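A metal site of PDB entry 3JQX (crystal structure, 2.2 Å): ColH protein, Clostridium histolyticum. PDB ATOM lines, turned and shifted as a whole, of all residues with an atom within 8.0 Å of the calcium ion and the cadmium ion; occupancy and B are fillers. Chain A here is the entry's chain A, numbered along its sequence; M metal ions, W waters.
The side-chain carboxylate of Asp 37 sits close to the backbone NH of Glu 33, 3.1 Å away. OH of Tyr 111 sits close to OD2 of Asp 39 (2.6 Å). The backbone NH of Leu 101 is in hydrogen-bond range of the backbone carbonyl oxygen of Asp 39 (2.8 Å). The backbone carbonyl oxygen (O) of Asn 12 sits at hydrogen-bond distance from the backbone NH (N) of Tyr 40 (2.9 Å). The side-chain amide nitrogen of Asn 12 lies within hydrogen-bond range of the side-chain hydroxyl of Ser 19 (3.3 Å). OG1 of Thr 17 lies within hydrogen-bond range of N of Asn 13. OE1 of Glu 8 lies close to OH of Tyr 111 (3.4 Å). The backbone NH (N) of Glu 8 is in hydrogen-bond range of the backbone carbonyl oxygen (O) of Ser 29 (3.1 Å).
Five residues have an atom within 4 Å of the cadmium ion: Glu 8, Glu 10, Thr 31, Asp 37 and Asp 39. The nearest printed residue that does not touch the cadmium ion is Ile 32 (4.3 Å).
The calcium ion is bound by OD1 of Asp 37 (2.3 Å), OD1 of Asp 39 (2.4 Å), OD1 of Asn 12 (2.4 Å), O of Gln 38 (2.4 Å), OE2 of Glu 10 (2.5 Å), OD1 of Asn 13 (2.6 Å) and OE1 of Glu 10 (2.7 Å). The calcium ion has seven donor atoms within binding distance.
The cadmium ion is bound by OD2 of Asp 37, O of Thr 31, OD1 of Asp 39, OE2 of Glu 10, OD2 of Asp 39, OE1 of Glu 8 and OE2 of Glu 8. The cadmium ion has seven donor atoms within binding distance.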
ATOM      1  N   GLU A   8       1.314  21.599   5.358  1.00  0.00           N
ATOM      2  CA  GLU A   8       2.061  22.787   4.941  1.00  0.00           C
ATOM      3  C   GLU A   8       1.748  23.954   5.921  1.00  0.00           C
ATOM      4  O   GLU A   8       0.727  23.946   6.631  1.00  0.00           O
ATOM      5  CB  GLU A   8       1.745  23.182   3.496  1.00  0.00           C
ATOM      6  CG  GLU A   8       0.270  23.538   3.337  1.00  0.00           C
ATOM      7  CD  GLU A   8      -0.089  24.226   2.027  1.00  0.00           C
ATOM      8  OE1 GLU A   8       0.794  24.704   1.296  1.00  0.00           O
ATOM      9  OE2 GLU A   8      -1.294  24.279   1.748  1.00  0.00           O
ATOM     10  N   LYS A   9       2.618  24.940   5.946  1.00  0.00           N
ATOM     11  CA  LYS A   9       2.474  26.087   6.870  1.00  0.00           C
ATOM     12  C   LYS A   9       2.702  27.340   6.022  1.00  0.00           C
ATOM     13  O   LYS A   9       3.825  27.644   5.664  1.00  0.00           O
ATOM     14  CB  LYS A   9       3.492  25.970   8.024  1.00  0.00           C
ATOM     15  CG  LYS A   9       3.513  27.134   9.010  1.00  0.00           C
ATOM     16  CD  LYS A   9       2.260  27.182   9.885  1.00  0.00           C
ATOM     17  CE  LYS A   9       2.294  28.359  10.931  1.00  0.00           C
ATOM     18  NZ  LYS A   9       0.889  28.719  11.490  1.00  0.00           N
ATOM     19  N   GLU A  10       1.623  28.021   5.660  1.00  0.00           N
ATOM     20  CA  GLU A  10       1.678  29.240   4.833  1.00  0.00           C
ATOM     21  C   GLU A  10       2.231  30.436   5.630  1.00  0.00           C
ATOM     22  O   GLU A  10       1.972  30.551   6.806  1.00  0.00           O
ATOM     23  CB  GLU A  10       0.274  29.559   4.260  1.00  0.00           C
ATOM     24  CG  GLU A  10      -0.272  28.529   3.236  1.00  0.00           C
ATOM     25  CD  GLU A  10       0.458  28.545   1.850  1.00  0.00           C
ATOM     26  OE1 GLU A  10       1.270  29.460   1.585  1.00  0.00           O
ATOM     27  OE2 GLU A  10       0.213  27.636   1.009  1.00  0.00           O
ATOM     28  N   PRO A  11       2.993  31.341   4.988  1.00  0.00           N
ATOM     29  CA  PRO A  11       3.445  31.368   3.589  1.00  0.00           C
ATOM     30  C   PRO A  11       4.591  30.354   3.366  1.00  0.00           C
ATOM     31  O   PRO A  11       5.454  30.204   4.201  1.00  0.00           O
ATOM     32  CB  PRO A  11       3.964  32.807   3.439  1.00  0.00           C
ATOM     33  CG  PRO A  11       4.606  33.076   4.831  1.00  0.00           C
ATOM     34  CD  PRO A  11       3.519  32.470   5.771  1.00  0.00           C
ATOM     35  N   ASN A  12       4.512  29.571   2.300  1.00  0.00           N
ATOM     36  CA  ASN A  12       5.563  28.640   1.967  1.00  0.00           C
ATOM     37  C   ASN A  12       5.865  28.796   0.470  1.00  0.00           C
ATOM     38  O   ASN A  12       6.183  27.810  -0.215  1.00  0.00           O
ATOM     39  CB  ASN A  12       5.212  27.210   2.344  1.00  0.00           C
ATOM     40  CG  ASN A  12       3.929  26.660   1.633  1.00  0.00           C
ATOM     41  OD1 ASN A  12       3.242  27.370   0.897  1.00  0.00           O
ATOM     42  ND2 ASN A  12       3.663  25.345   1.820  1.00  0.00           N
ATOM     43  N   ASN A  13       5.676  30.053   0.005  1.00  0.00           N
ATOM     44  CA  ASN A  13       5.714  30.423  -1.416  1.00  0.00           C
ATOM     45  C   ASN A  13       7.106  30.607  -2.011  1.00  0.00           C
ATOM     46  O   ASN A  13       7.227  31.047  -3.170  1.00  0.00           O
ATOM     47  CB  ASN A  13       4.808  31.630  -1.739  1.00  0.00           C
ATOM     48  CG  ASN A  13       3.318  31.240  -1.780  1.00  0.00           C
ATOM     49  OD1 ASN A  13       2.828  30.651  -0.791  1.00  0.00           O
ATOM     50  ND2 ASN A  13       2.586  31.545  -2.941  1.00  0.00           N
ATOM     51  N   SER A  14       8.151  30.196  -1.269  1.00  0.00           N
ATOM     52  CA  SER A  14       9.503  30.181  -1.803  1.00  0.00           C
ATOM     53  C   SER A  14      10.292  29.137  -1.042  1.00  0.00           C
ATOM     54  O   SER A  14       9.811  28.663  -0.013  1.00  0.00           O
ATOM     55  CB  SER A  14      10.112  31.583  -1.663  1.00  0.00           C
ATOM     56  OG  SER A  14      10.215  31.910  -0.286  1.00  0.00           O
ATOM     57  N   THR A  17      11.003  30.016   2.439  1.00  0.00           N
ATOM     58  CA  THR A  17       9.922  29.747   3.400  1.00  0.00           C
ATOM     59  C   THR A  17       9.316  28.305   3.342  1.00  0.00           C
ATOM     60  O   THR A  17       8.279  28.066   3.926  1.00  0.00           O
ATOM     61  CB  THR A  17       8.815  30.821   3.294  1.00  0.00           C
ATOM     62  OG1 THR A  17       8.295  30.843   1.978  1.00  0.00           O
ATOM     63  CG2 THR A  17       9.371  32.225   3.581  1.00  0.00           C
ATOM     64  N   SER A  19       7.919  24.693   3.896  1.00  0.00           N
ATOM     65  CA  SER A  19       7.500  23.861   5.059  1.00  0.00           C
ATOM     66  C   SER A  19       8.294  22.572   5.154  1.00  0.00           C
ATOM     67  O   SER A  19       8.433  21.807   4.173  1.00  0.00           O
ATOM     68  CB  SER A  19       5.989  23.497   4.945  1.00  0.00           C
ATOM     69  OG  SER A  19       5.189  24.657   4.656  1.00  0.00           O
ATOM     70  N   SER A  29      -0.261  16.997   4.309  1.00  0.00           N
ATOM     71  CA  SER A  29      -1.469  17.506   3.659  1.00  0.00           C
ATOM     72  C   SER A  29      -1.246  18.928   3.227  1.00  0.00           C
ATOM     73  O   SER A  29      -0.569  19.642   3.886  1.00  0.00           O
ATOM     74  CB  SER A  29      -2.572  17.634   4.708  1.00  0.00           C
ATOM     75  OG  SER A  29      -3.142  16.381   4.821  1.00  0.00           O
ATOM     76  N   GLY A  30      -1.870  19.357   2.156  1.00  0.00           N
ATOM     77  CA  GLY A  30      -1.898  20.782   1.847  1.00  0.00           C
ATOM     78  C   GLY A  30      -2.952  20.960   0.819  1.00  0.00           C
ATOM     79  O   GLY A  30      -3.672  19.999   0.449  1.00  0.00           O
ATOM     80  N   THR A  31      -3.014  22.190   0.304  1.00  0.00           N
ATOM     81  CA  THR A  31      -3.952  22.538  -0.726  1.00  0.00           C
ATOM     82  C   THR A  31      -3.273  23.517  -1.619  1.00  0.00           C
ATOM     83  O   THR A  31      -2.758  24.447  -1.095  1.00  0.00           O
ATOM     84  CB  THR A  31      -5.118  23.330  -0.130  1.00  0.00           C
ATOM     85  OG1 THR A  31      -5.921  22.447   0.654  1.00  0.00           O
ATOM     86  CG2 THR A  31      -5.991  23.897  -1.275  1.00  0.00           C
ATOM     87  N   ILE A  32      -3.297  23.325  -2.950  1.00  0.00           N
ATOM     88  CA  ILE A  32      -2.890  24.384  -3.882  1.00  0.00           C
ATOM     89  C   ILE A  32      -4.136  25.284  -4.095  1.00  0.00           C
ATOM     90  O   ILE A  32      -5.063  24.832  -4.792  1.00  0.00           O
ATOM     91  CB  ILE A  32      -2.333  23.862  -5.267  1.00  0.00           C
ATOM     92  CG1 ILE A  32      -1.332  22.709  -5.085  1.00  0.00           C
ATOM     93  CG2 ILE A  32      -1.647  25.061  -6.059  1.00  0.00           C
ATOM     94  CD1 ILE A  32      -0.822  22.036  -6.362  1.00  0.00           C
ATOM     95  N   GLU A  33      -4.147  26.511  -3.522  1.00  0.00           N
ATOM     96  CA  GLU A  33      -5.368  27.322  -3.400  1.00  0.00           C
ATOM     97  C   GLU A  33      -5.976  27.776  -4.698  1.00  0.00           C
ATOM     98  O   GLU A  33      -7.186  27.949  -4.819  1.00  0.00           O
ATOM     99  CB  GLU A  33      -5.205  28.501  -2.415  1.00  0.00           C
ATOM    100  CG  GLU A  33      -4.888  28.052  -0.973  1.00  0.00           C
ATOM    101  CD  GLU A  33      -6.126  27.831  -0.045  1.00  0.00           C
ATOM    102  OE1 GLU A  33      -7.223  28.393  -0.312  1.00  0.00           O
ATOM    103  OE2 GLU A  33      -5.985  27.086   0.982  1.00  0.00           O
ATOM    104  N   ASN A  34      -5.106  27.936  -5.687  1.00  0.00           N
ATOM    105  CA  ASN A  34      -5.396  28.410  -7.011  1.00  0.00           C
ATOM    106  C   ASN A  34      -3.986  28.442  -7.647  1.00  0.00           C
ATOM    107  O   ASN A  34      -3.039  28.163  -6.936  1.00  0.00           O
ATOM    108  CB  ASN A  34      -6.113  29.764  -7.048  1.00  0.00           C
ATOM    109  CG  ASN A  34      -5.390  30.875  -6.271  1.00  0.00           C
ATOM    110  OD1 ASN A  34      -4.220  31.088  -6.400  1.00  0.00           O
ATOM    111  ND2 ASN A  34      -6.147  31.617  -5.494  1.00  0.00           N
ATOM    112  N   SER A  36      -1.934  30.700  -8.454  1.00  0.00           N
ATOM    113  CA  SER A  36      -0.970  31.623  -7.827  1.00  0.00           C
ATOM    114  C   SER A  36      -0.338  31.121  -6.522  1.00  0.00           C
ATOM    115  O   SER A  36       0.585  31.730  -5.988  1.00  0.00           O
ATOM    116  CB  SER A  36      -1.631  33.002  -7.594  1.00  0.00           C
ATOM    117  OG  SER A  36      -1.917  33.620  -8.875  1.00  0.00           O
ATOM    118  N   ASP A  37      -0.873  30.027  -5.983  1.00  0.00           N
ATOM    119  CA  ASP A  37      -0.281  29.423  -4.818  1.00  0.00           C
ATOM    120  C   ASP A  37       0.878  28.479  -5.180  1.00  0.00           C
ATOM    121  O   ASP A  37       0.666  27.425  -5.748  1.00  0.00           O
ATOM    122  CB  ASP A  37      -1.359  28.629  -4.091  1.00  0.00           C
ATOM    123  CG  ASP A  37      -0.906  28.177  -2.713  1.00  0.00           C
ATOM    124  OD1 ASP A  37       0.017  28.804  -2.103  1.00  0.00           O
ATOM    125  OD2 ASP A  37      -1.446  27.177  -2.253  1.00  0.00           O
ATOM    126  N   GLN A  38       2.108  28.845  -4.802  1.00  0.00           N
ATOM    127  CA  GLN A  38       3.271  27.980  -4.937  1.00  0.00           C
ATOM    128  C   GLN A  38       3.527  27.298  -3.579  1.00  0.00           C
ATOM    129  O   GLN A  38       3.535  27.982  -2.566  1.00  0.00           O
ATOM    130  CB  GLN A  38       4.492  28.791  -5.395  1.00  0.00           C
ATOM    131  CG  GLN A  38       4.205  29.718  -6.532  1.00  0.00           C
ATOM    132  CD  GLN A  38       4.194  28.964  -7.857  1.00  0.00           C
ATOM    133  OE1 GLN A  38       4.934  27.988  -8.043  1.00  0.00           O
ATOM    134  NE2 GLN A  38       3.308  29.357  -8.776  1.00  0.00           N
ATOM    135  N   ASP A  39       3.699  25.962  -3.540  1.00  0.00           N
ATOM    136  CA  ASP A  39       3.950  25.282  -2.270  1.00  0.00           C
ATOM    137  C   ASP A  39       5.325  24.673  -2.242  1.00  0.00           C
ATOM    138  O   ASP A  39       5.611  23.754  -3.023  1.00  0.00           O
ATOM    139  CB  ASP A  39       2.898  24.214  -1.980  1.00  0.00           C
ATOM    140  CG  ASP A  39       1.542  24.797  -1.642  1.00  0.00           C
ATOM    141  OD1 ASP A  39       1.450  26.022  -1.389  1.00  0.00           O
ATOM    142  OD2 ASP A  39       0.555  24.042  -1.612  1.00  0.00           O
ATOM    143  N   TYR A  40       6.204  25.202  -1.387  1.00  0.00           N
ATOM    144  CA  TYR A  40       7.556  24.587  -1.222  1.00  0.00           C
ATOM    145  C   TYR A  40       7.675  23.873   0.095  1.00  0.00           C
ATOM    146  O   TYR A  40       7.174  24.335   1.091  1.00  0.00           O
ATOM    147  CB  TYR A  40       8.681  25.635  -1.324  1.00  0.00           C
ATOM    148  CG  TYR A  40       8.820  26.360  -2.646  1.00  0.00           C
ATOM    149  CD1 TYR A  40       7.967  27.386  -3.008  1.00  0.00           C
ATOM    150  CD2 TYR A  40       9.849  26.045  -3.519  1.00  0.00           C
ATOM    151  CE1 TYR A  40       8.154  28.136  -4.273  1.00  0.00           C
ATOM    152  CE2 TYR A  40      10.046  26.794  -4.763  1.00  0.00           C
ATOM    153  CZ  TYR A  40       9.192  27.820  -5.126  1.00  0.00           C
ATOM    154  OH  TYR A  40       9.405  28.526  -6.360  1.00  0.00           O
ATOM    155  N   PHE A  41       8.352  22.715   0.029  1.00  0.00           N
ATOM    156  CA  PHE A  41       8.648  21.844   1.133  1.00  0.00           C
ATOM    157  C   PHE A  41      10.128  21.533   1.120  1.00  0.00           C
ATOM    158  O   PHE A  41      10.793  21.748   0.123  1.00  0.00           O
ATOM    159  CB  PHE A  41       7.853  20.528   1.007  1.00  0.00           C
ATOM    160  CG  PHE A  41       6.346  20.771   0.960  1.00  0.00           C
ATOM    161  CD1 PHE A  41       5.556  20.770   2.140  1.00  0.00           C
ATOM    162  CD2 PHE A  41       5.732  21.080  -0.236  1.00  0.00           C
ATOM    163  CE1 PHE A  41       4.206  21.079   2.102  1.00  0.00           C
ATOM    164  CE2 PHE A  41       4.362  21.338  -0.271  1.00  0.00           C
ATOM    165  CZ  PHE A  41       3.607  21.337   0.901  1.00  0.00           C
ATOM    166  N   LEU A 101       6.110  22.447  -5.434  1.00  0.00           N
ATOM    167  CA  LEU A 101       4.830  22.013  -5.991  1.00  0.00           C
ATOM    168  C   LEU A 101       4.007  23.205  -6.462  1.00  0.00           C
ATOM    169  O   LEU A 101       3.907  24.224  -5.786  1.00  0.00           O
ATOM    170  CB  LEU A 101       4.042  21.288  -4.911  1.00  0.00           C
ATOM    171  CG  LEU A 101       2.667  20.748  -5.238  1.00  0.00           C
ATOM    172  CD1 LEU A 101       2.758  19.432  -6.117  1.00  0.00           C
ATOM    173  CD2 LEU A 101       2.085  20.386  -3.922  1.00  0.00           C
ATOM    174  N   MET A 109      -6.740  22.651  -5.614  1.00  0.00           N
ATOM    175  CA  MET A 109      -6.245  21.289  -5.410  1.00  0.00           C
ATOM    176  C   MET A 109      -5.744  20.831  -4.011  1.00  0.00           C
ATOM    177  O   MET A 109      -4.617  21.121  -3.624  1.00  0.00           O
ATOM    178  CB  MET A 109      -5.152  20.937  -6.438  1.00  0.00           C
ATOM    179  CG  MET A 109      -5.146  19.414  -6.664  1.00  0.00           C
ATOM    180  SD  MET A 109      -3.782  18.900  -7.645  1.00  0.00           S
ATOM    181  CE  MET A 109      -4.338  19.313  -9.289  1.00  0.00           C
ATOM    182  N   TYR A 111      -4.043  17.936  -1.712  1.00  0.00           N
ATOM    183  CA  TYR A 111      -3.097  16.926  -2.014  1.00  0.00           C
ATOM    184  C   TYR A 111      -2.532  16.337  -0.724  1.00  0.00           C
ATOM    185  O   TYR A 111      -2.798  16.805   0.405  1.00  0.00           O
ATOM    186  CB  TYR A 111      -1.989  17.477  -2.917  1.00  0.00           C
ATOM    187  CG  TYR A 111      -1.223  18.605  -2.231  1.00  0.00           C
ATOM    188  CD1 TYR A 111      -0.277  18.342  -1.197  1.00  0.00           C
ATOM    189  CD2 TYR A 111      -1.492  19.901  -2.548  1.00  0.00           C
ATOM    190  CE1 TYR A 111       0.418  19.421  -0.552  1.00  0.00           C
ATOM    191  CE2 TYR A 111      -0.829  20.954  -1.908  1.00  0.00           C
ATOM    192  CZ  TYR A 111       0.097  20.713  -0.938  1.00  0.00           C
ATOM    193  OH  TYR A 111       0.704  21.781  -0.370  1.00  0.00           O
HETATM  194 CA    CA M   1       1.837  28.301  -0.840  1.00  0.00          CA
HETATM  195 CD    CD M   2      -0.839  25.799  -0.384  1.00  0.00          CD
HETATM  196  O   HOH W   1      -3.135  26.964   1.415  1.00  0.00           O
